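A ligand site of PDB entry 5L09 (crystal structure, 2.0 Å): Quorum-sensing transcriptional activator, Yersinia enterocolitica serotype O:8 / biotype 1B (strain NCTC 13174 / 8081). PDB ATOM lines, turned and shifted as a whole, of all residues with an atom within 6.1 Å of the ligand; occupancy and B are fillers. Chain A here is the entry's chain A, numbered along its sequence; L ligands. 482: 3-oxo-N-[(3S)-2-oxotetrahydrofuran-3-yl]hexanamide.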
ATOM      1  N   SER A  32      23.487   7.661  -7.552  1.00  0.00           N
ATOM      2  CA  SER A  32      22.161   7.313  -7.072  1.00  0.00           C
ATOM      3  C   SER A  32      21.387   8.596  -6.813  1.00  0.00           C
ATOM      4  O   SER A  32      21.822   9.412  -6.002  1.00  0.00           O
ATOM      5  CB  SER A  32      22.217   6.478  -5.796  1.00  0.00           C
ATOM      6  OG  SER A  32      20.883   6.190  -5.401  1.00  0.00           O
ATOM      7  N   TYR A  33      20.256   8.748  -7.491  1.00  0.00           N
ATOM      8  CA  TYR A  33      19.280   9.774  -7.197  1.00  0.00           C
ATOM      9  C   TYR A  33      18.291   9.153  -6.216  1.00  0.00           C
ATOM     10  O   TYR A  33      17.548   8.231  -6.561  1.00  0.00           O
ATOM     11  CB  TYR A  33      18.606  10.244  -8.487  1.00  0.00           C
ATOM     12  CG  TYR A  33      17.366  11.135  -8.332  1.00  0.00           C
ATOM     13  CD1 TYR A  33      17.449  12.425  -7.822  1.00  0.00           C
ATOM     14  CD2 TYR A  33      16.125  10.686  -8.750  1.00  0.00           C
ATOM     15  CE1 TYR A  33      16.305  13.252  -7.692  1.00  0.00           C
ATOM     16  CE2 TYR A  33      14.985  11.484  -8.630  1.00  0.00           C
ATOM     17  CZ  TYR A  33      15.081  12.771  -8.114  1.00  0.00           C
ATOM     18  OH  TYR A  33      13.949  13.534  -7.996  1.00  0.00           O
ATOM     19  N   LEU A  34      18.281   9.648  -4.973  1.00  0.00           N
ATOM     20  CA  LEU A  34      17.443   9.105  -3.918  1.00  0.00           C
ATOM     21  C   LEU A  34      16.529  10.214  -3.412  1.00  0.00           C
ATOM     22  O   LEU A  34      17.005  11.270  -2.978  1.00  0.00           O
ATOM     23  CB  LEU A  34      18.309   8.517  -2.777  1.00  0.00           C
ATOM     24  CG  LEU A  34      17.530   7.818  -1.623  1.00  0.00           C
ATOM     25  CD1 LEU A  34      18.430   6.800  -0.892  1.00  0.00           C
ATOM     26  CD2 LEU A  34      16.909   8.809  -0.593  1.00  0.00           C
ATOM     27  N   ILE A  46      14.550   5.387  -5.578  1.00  0.00           N
ATOM     28  CA  ILE A  46      15.977   5.270  -5.869  1.00  0.00           C
ATOM     29  C   ILE A  46      16.148   5.028  -7.366  1.00  0.00           C
ATOM     30  O   ILE A  46      15.668   4.012  -7.888  1.00  0.00           O
ATOM     31  CB  ILE A  46      16.657   4.143  -5.069  1.00  0.00           C
ATOM     32  CG1 ILE A  46      16.654   4.443  -3.572  1.00  0.00           C
ATOM     33  CG2 ILE A  46      18.101   3.909  -5.555  1.00  0.00           C
ATOM     34  CD1 ILE A  46      17.158   3.267  -2.683  1.00  0.00           C
ATOM     35  N   SER A  48      19.287   4.664  -9.984  1.00  0.00           N
ATOM     36  CA  SER A  48      20.711   4.457  -9.707  1.00  0.00           C
ATOM     37  C   SER A  48      21.318   3.461 -10.682  1.00  0.00           C
ATOM     38  O   SER A  48      20.637   2.542 -11.146  1.00  0.00           O
ATOM     39  CB  SER A  48      20.897   3.945  -8.254  1.00  0.00           C
ATOM     40  OG  SER A  48      22.251   3.660  -7.959  1.00  0.00           O
ATOM     41  N   TYR A  50      24.113   2.019  -9.290  1.00  0.00           N
ATOM     42  CA  TYR A  50      24.874   1.220  -8.325  1.00  0.00           C
ATOM     43  C   TYR A  50      24.674  -0.265  -8.642  1.00  0.00           C
ATOM     44  O   TYR A  50      23.665  -0.644  -9.226  1.00  0.00           O
ATOM     45  CB  TYR A  50      24.396   1.504  -6.888  1.00  0.00           C
ATOM     46  CG  TYR A  50      24.905   2.798  -6.237  1.00  0.00           C
ATOM     47  CD1 TYR A  50      25.517   3.805  -6.990  1.00  0.00           C
ATOM     48  CD2 TYR A  50      24.750   3.007  -4.862  1.00  0.00           C
ATOM     49  CE1 TYR A  50      25.992   4.996  -6.368  1.00  0.00           C
ATOM     50  CE2 TYR A  50      25.207   4.177  -4.247  1.00  0.00           C
ATOM     51  CZ  TYR A  50      25.823   5.170  -4.998  1.00  0.00           C
ATOM     52  OH  TYR A  50      26.265   6.330  -4.369  1.00  0.00           O
ATOM     53  N   TRP A  54      23.533  -4.456  -4.362  1.00  0.00           N
ATOM     54  CA  TRP A  54      23.627  -3.475  -3.286  1.00  0.00           C
ATOM     55  C   TRP A  54      22.329  -2.679  -3.157  1.00  0.00           C
ATOM     56  O   TRP A  54      21.807  -2.518  -2.048  1.00  0.00           O
ATOM     57  CB  TRP A  54      24.834  -2.557  -3.520  1.00  0.00           C
ATOM     58  CG  TRP A  54      25.010  -1.451  -2.527  1.00  0.00           C
ATOM     59  CD1 TRP A  54      25.256  -0.129  -2.818  1.00  0.00           C
ATOM     60  CD2 TRP A  54      24.969  -1.536  -1.098  1.00  0.00           C
ATOM     61  NE1 TRP A  54      25.363   0.606  -1.659  1.00  0.00           N
ATOM     62  CE2 TRP A  54      25.177  -0.231  -0.584  1.00  0.00           C
ATOM     63  CE3 TRP A  54      24.759  -2.596  -0.194  1.00  0.00           C
ATOM     64  CZ2 TRP A  54      25.205   0.045   0.777  1.00  0.00           C
ATOM     65  CZ3 TRP A  54      24.774  -2.317   1.162  1.00  0.00           C
ATOM     66  CH2 TRP A  54      25.004  -1.018   1.635  1.00  0.00           C
ATOM     67  N   VAL A  55      21.788  -2.208  -4.287  1.00  0.00           N
ATOM     68  CA  VAL A  55      20.521  -1.491  -4.268  1.00  0.00           C
ATOM     69  C   VAL A  55      19.429  -2.344  -3.623  1.00  0.00           C
ATOM     70  O   VAL A  55      18.681  -1.873  -2.753  1.00  0.00           O
ATOM     71  CB  VAL A  55      20.120  -1.062  -5.690  1.00  0.00           C
ATOM     72  CG1 VAL A  55      18.694  -0.561  -5.708  1.00  0.00           C
ATOM     73  CG2 VAL A  55      21.103  -0.005  -6.231  1.00  0.00           C
ATOM     74  N   TYR A  58      20.017  -2.594   0.090  1.00  0.00           N
ATOM     75  CA  TYR A  58      19.821  -1.302   0.749  1.00  0.00           C
ATOM     76  C   TYR A  58      18.333  -1.011   0.915  1.00  0.00           C
ATOM     77  O   TYR A  58      17.901  -0.519   1.965  1.00  0.00           O
ATOM     78  CB  TYR A  58      20.525  -0.229  -0.107  1.00  0.00           C
ATOM     79  CG  TYR A  58      20.624   1.184   0.457  1.00  0.00           C
ATOM     80  CD1 TYR A  58      21.816   1.643   1.010  1.00  0.00           C
ATOM     81  CD2 TYR A  58      19.549   2.050   0.384  1.00  0.00           C
ATOM     82  CE1 TYR A  58      21.917   2.946   1.521  1.00  0.00           C
ATOM     83  CE2 TYR A  58      19.649   3.363   0.864  1.00  0.00           C
ATOM     84  CZ  TYR A  58      20.840   3.801   1.429  1.00  0.00           C
ATOM     85  OH  TYR A  58      20.941   5.098   1.897  1.00  0.00           O
ATOM     86  N   ASP A  67      22.035   5.576   7.060  1.00  0.00           N
ATOM     87  CA  ASP A  67      23.116   5.904   6.131  1.00  0.00           C
ATOM     88  C   ASP A  67      23.703   7.261   6.514  1.00  0.00           C
ATOM     89  O   ASP A  67      22.990   8.274   6.450  1.00  0.00           O
ATOM     90  CB  ASP A  67      22.567   5.939   4.700  1.00  0.00           C
ATOM     91  CG  ASP A  67      23.654   6.139   3.640  1.00  0.00           C
ATOM     92  OD1 ASP A  67      24.763   6.638   3.946  1.00  0.00           O
ATOM     93  OD2 ASP A  67      23.377   5.791   2.465  1.00  0.00           O
ATOM     94  N   PRO A  68      24.977   7.324   6.921  1.00  0.00           N
ATOM     95  CA  PRO A  68      25.573   8.629   7.290  1.00  0.00           C
ATOM     96  C   PRO A  68      25.369   9.727   6.255  1.00  0.00           C
ATOM     97  O   PRO A  68      25.219  10.900   6.638  1.00  0.00           O
ATOM     98  CB  PRO A  68      27.064   8.294   7.458  1.00  0.00           C
ATOM     99  CG  PRO A  68      27.108   6.840   7.781  1.00  0.00           C
ATOM    100  CD  PRO A  68      25.957   6.235   6.988  1.00  0.00           C
ATOM    101  N   VAL A  69      25.367   9.413   4.948  1.00  0.00           N
ATOM    102  CA  VAL A  69      25.258  10.536   4.004  1.00  0.00           C
ATOM    103  C   VAL A  69      23.834  11.052   3.931  1.00  0.00           C
ATOM    104  O   VAL A  69      23.631  12.256   3.757  1.00  0.00           O
ATOM    105  CB  VAL A  69      25.803  10.166   2.606  1.00  0.00           C
ATOM    106  CG1 VAL A  69      27.206   9.538   2.729  1.00  0.00           C
ATOM    107  CG2 VAL A  69      24.850   9.283   1.799  1.00  0.00           C
ATOM    108  N   ILE A  70      22.832  10.179   4.098  1.00  0.00           N
ATOM    109  CA  ILE A  70      21.437  10.621   4.130  1.00  0.00           C
ATOM    110  C   ILE A  70      21.164  11.393   5.418  1.00  0.00           C
ATOM    111  O   ILE A  70      20.495  12.427   5.413  1.00  0.00           O
ATOM    112  CB  ILE A  70      20.485   9.418   3.989  1.00  0.00           C
ATOM    113  CG1 ILE A  70      20.760   8.651   2.678  1.00  0.00           C
ATOM    114  CG2 ILE A  70      19.028   9.851   4.097  1.00  0.00           C
ATOM    115  CD1 ILE A  70      20.678   9.561   1.415  1.00  0.00           C
ATOM    116  N   TRP A  82      31.974  12.618   1.211  1.00  0.00           N
ATOM    117  CA  TRP A  82      31.676  11.639   2.253  1.00  0.00           C
ATOM    118  C   TRP A  82      32.769  11.553   3.297  1.00  0.00           C
ATOM    119  O   TRP A  82      32.561  10.911   4.323  1.00  0.00           O
ATOM    120  CB  TRP A  82      31.460  10.269   1.657  1.00  0.00           C
ATOM    121  CG  TRP A  82      30.278  10.200   0.718  1.00  0.00           C
ATOM    122  CD1 TRP A  82      29.304  11.144   0.546  1.00  0.00           C
ATOM    123  CD2 TRP A  82      29.984   9.134  -0.165  1.00  0.00           C
ATOM    124  NE1 TRP A  82      28.418  10.729  -0.424  1.00  0.00           N
ATOM    125  CE2 TRP A  82      28.806   9.485  -0.865  1.00  0.00           C
ATOM    126  CE3 TRP A  82      30.599   7.905  -0.442  1.00  0.00           C
ATOM    127  CZ2 TRP A  82      28.224   8.648  -1.829  1.00  0.00           C
ATOM    128  CZ3 TRP A  82      30.030   7.066  -1.402  1.00  0.00           C
ATOM    129  CH2 TRP A  82      28.836   7.431  -2.070  1.00  0.00           C
ATOM    130  N   VAL A  97      26.551   0.786   7.027  1.00  0.00           N
ATOM    131  CA  VAL A  97      26.280   1.055   5.614  1.00  0.00           C
ATOM    132  C   VAL A  97      27.592   1.184   4.856  1.00  0.00           C
ATOM    133  O   VAL A  97      27.756   0.607   3.770  1.00  0.00           O
ATOM    134  CB  VAL A  97      25.386   2.304   5.434  1.00  0.00           C
ATOM    135  CG1 VAL A  97      25.453   2.784   4.008  1.00  0.00           C
ATOM    136  CG2 VAL A  97      23.928   1.951   5.791  1.00  0.00           C
ATOM    137  N   PHE A  98      28.573   1.887   5.418  1.00  0.00           N
ATOM    138  CA  PHE A  98      29.831   2.031   4.670  1.00  0.00           C
ATOM    139  C   PHE A  98      30.589   0.710   4.615  1.00  0.00           C
ATOM    140  O   PHE A  98      31.216   0.398   3.585  1.00  0.00           O
ATOM    141  CB  PHE A  98      30.683   3.146   5.268  1.00  0.00           C
ATOM    142  CG  PHE A  98      30.371   4.491   4.669  1.00  0.00           C
ATOM    143  CD1 PHE A  98      31.218   5.079   3.759  1.00  0.00           C
ATOM    144  CD2 PHE A  98      29.177   5.151   4.993  1.00  0.00           C
ATOM    145  CE1 PHE A  98      30.932   6.309   3.184  1.00  0.00           C
ATOM    146  CE2 PHE A  98      28.884   6.406   4.452  1.00  0.00           C
ATOM    147  CZ  PHE A  98      29.754   6.985   3.538  1.00  0.00           C
ATOM    148  N   ALA A 101      28.904  -1.234   1.917  1.00  0.00           N
ATOM    149  CA  ALA A 101      29.156  -0.607   0.624  1.00  0.00           C
ATOM    150  C   ALA A 101      30.573  -0.881   0.123  1.00  0.00           C
ATOM    151  O   ALA A 101      30.796  -0.959  -1.087  1.00  0.00           O
ATOM    152  CB  ALA A 101      28.929   0.907   0.719  1.00  0.00           C
ATOM    153  N   ILE A 106      32.133   0.922  -3.238  1.00  0.00           N
ATOM    154  CA  ILE A 106      31.511   2.240  -3.053  1.00  0.00           C
ATOM    155  C   ILE A 106      32.085   2.784  -1.752  1.00  0.00           C
ATOM    156  O   ILE A 106      31.583   2.525  -0.659  1.00  0.00           O
ATOM    157  CB  ILE A 106      29.989   2.159  -3.040  1.00  0.00           C
ATOM    158  CG1 ILE A 106      29.488   1.730  -4.426  1.00  0.00           C
ATOM    159  CG2 ILE A 106      29.359   3.512  -2.629  1.00  0.00           C
ATOM    160  CD1 ILE A 106      28.023   1.486  -4.475  1.00  0.00           C
ATOM    161  N   VAL A 107      33.174   3.541  -1.872  1.00  0.00           N
ATOM    162  CA  VAL A 107      33.949   3.976  -0.717  1.00  0.00           C
ATOM    163  C   VAL A 107      34.117   5.483  -0.671  1.00  0.00           C
ATOM    164  O   VAL A 107      34.001   6.102   0.395  1.00  0.00           O
ATOM    165  CB  VAL A 107      35.335   3.284  -0.710  1.00  0.00           C
ATOM    166  CG1 VAL A 107      36.154   3.804   0.417  1.00  0.00           C
ATOM    167  CG2 VAL A 107      35.160   1.765  -0.603  1.00  0.00           C
ATOM    168  N   THR A 111      27.759  13.848  -1.908  1.00  0.00           N
ATOM    169  CA  THR A 111      26.301  13.954  -1.912  1.00  0.00           C
ATOM    170  C   THR A 111      25.897  15.388  -2.195  1.00  0.00           C
ATOM    171  O   THR A 111      26.440  16.336  -1.593  1.00  0.00           O
ATOM    172  CB  THR A 111      25.730  13.445  -0.580  1.00  0.00           C
ATOM    173  OG1 THR A 111      25.891  12.019  -0.529  1.00  0.00           O
ATOM    174  CG2 THR A 111      24.197  13.829  -0.445  1.00  0.00           C
ATOM    175  N   THR A 123      18.472  13.680  -3.089  1.00  0.00           N
ATOM    176  CA  THR A 123      19.922  13.654  -3.078  1.00  0.00           C
ATOM    177  C   THR A 123      20.434  13.072  -4.373  1.00  0.00           C
ATOM    178  O   THR A 123      19.794  12.206  -4.976  1.00  0.00           O
ATOM    179  CB  THR A 123      20.505  12.814  -1.913  1.00  0.00           C
ATOM    180  OG1 THR A 123      19.933  11.496  -1.921  1.00  0.00           O
ATOM    181  CG2 THR A 123      20.239  13.490  -0.577  1.00  0.00           C
ATOM    182  N   ASN A 125      23.852  11.240  -5.151  1.00  0.00           N
ATOM    183  CA  ASN A 125      25.028  10.656  -4.522  1.00  0.00           C
ATOM    184  C   ASN A 125      25.889  10.070  -5.619  1.00  0.00           C
ATOM    185  O   ASN A 125      25.383   9.372  -6.497  1.00  0.00           O
ATOM    186  CB  ASN A 125      24.593   9.570  -3.529  1.00  0.00           C
ATOM    187  CG  ASN A 125      23.521  10.071  -2.601  1.00  0.00           C
ATOM    188  OD1 ASN A 125      23.809  10.828  -1.683  1.00  0.00           O
ATOM    189  ND2 ASN A 125      22.251   9.720  -2.883  1.00  0.00           N
ATOM    190  N   ILE A 126      27.190  10.361  -5.577  1.00  0.00           N
ATOM    191  CA  ILE A 126      28.052   9.968  -6.684  1.00  0.00           C
ATOM    192  C   ILE A 126      29.352   9.403  -6.126  1.00  0.00           C
ATOM    193  O   ILE A 126      29.879   9.899  -5.138  1.00  0.00           O
ATOM    194  CB  ILE A 126      28.355  11.145  -7.642  1.00  0.00           C
ATOM    195  CG1 ILE A 126      28.953  12.327  -6.862  1.00  0.00           C
ATOM    196  CG2 ILE A 126      27.089  11.559  -8.399  1.00  0.00           C
ATOM    197  CD1 ILE A 126      29.350  13.494  -7.767  1.00  0.00           C
HETATM  198  C15 482 L   1      21.489   2.414  -2.961  1.00  0.00           C
HETATM  199  C14 482 L   1      21.421   3.940  -2.974  1.00  0.00           C
HETATM  200  C13 482 L   1      22.105   4.523  -1.737  1.00  0.00           C
HETATM  201  C11 482 L   1      22.055   6.055  -1.793  1.00  0.00           C
HETATM  202  O12 482 L   1      21.458   6.621  -2.698  1.00  0.00           O
HETATM  203  C10 482 L   1      22.773   6.868  -0.752  1.00  0.00           C
HETATM  204  C8  482 L   1      24.239   6.530  -0.889  1.00  0.00           C
HETATM  205  O9  482 L   1      24.796   6.620  -1.983  1.00  0.00           O
HETATM  206  N7  482 L   1      24.880   6.113   0.191  1.00  0.00           N
HETATM  207  C1  482 L   1      26.262   5.702   0.030  1.00  0.00           C
HETATM  208  C5  482 L   1      27.104   5.939   1.276  1.00  0.00           C
HETATM  209  C4  482 L   1      28.196   4.851   1.212  1.00  0.00           C
HETATM  210  C2  482 L   1      26.433   4.230  -0.179  1.00  0.00           C
HETATM  211  O6  482 L   1      25.736   3.501  -0.856  1.00  0.00           O
HETATM  212  OAP 482 L   1      27.557   3.755   0.552  1.00  0.00           O
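A nitrogen (N7) of the ligand lies within hydrogen-bond range of the side-chain carboxylate (OD2) of Asp 67, 2.7 Å away. OG of Ser 32 is in hydrogen-bond range of O12 of the ligand. O9 of the ligand sits at hydrogen-bond distance from OH of Tyr 50 (2.8 Å). O6 of the ligand sits at hydrogen-bond distance from NE1 of Trp 54 (3.0 Å). ND2 of Asn 125 lies within hydrogen-bond range of O12 of the ligand (3.2 Å).
OD2 of Asp 67 sits at hydrogen-bond distance from OH of Tyr 58, at 2.6 Å. The backbone NH of Ser 32 lies within hydrogen-bond range of the backbone carbonyl oxygen of Asn 125. N of Tyr 50 is in hydrogen-bond range of OG of Ser 48 (2.8 Å). The backbone carbonyl oxygen of Ala 101 lies within hydrogen-bond range of the backbone NH of Ile 106 (3.2 Å). ND2 of Asn 125 is in hydrogen-bond range of OG1 of Thr 123. OD1 of Asn 125 sits at hydrogen-bond distance from OG1 of Thr 111 (2.7 Å). O of Leu 34 lies within hydrogen-bond range of N of Thr 123, at 2.8 Å. NE1 of Trp 82 sits at hydrogen-bond distance from OG1 of Thr 111 (2.8 Å).
Residues that only touch the ligand: Leu 34 (3.5 Å), Tyr 58 (3.5 Å), Val 69 (3.6 Å), Trp 82 (3.7 Å), Phe 98 (3.5 Å), Ala 101 (3.2 Å) and Ile 106 (3.7 Å). Hydrophobic or aromatic side chains that line the ligand: Leu 34, Tyr 50, Trp 54, Tyr 58, Val 69, Trp 82, Phe 98, Ala 101 and Ile 106. Of the 23 residues printed, 12 come within 4 Å of the ligand.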
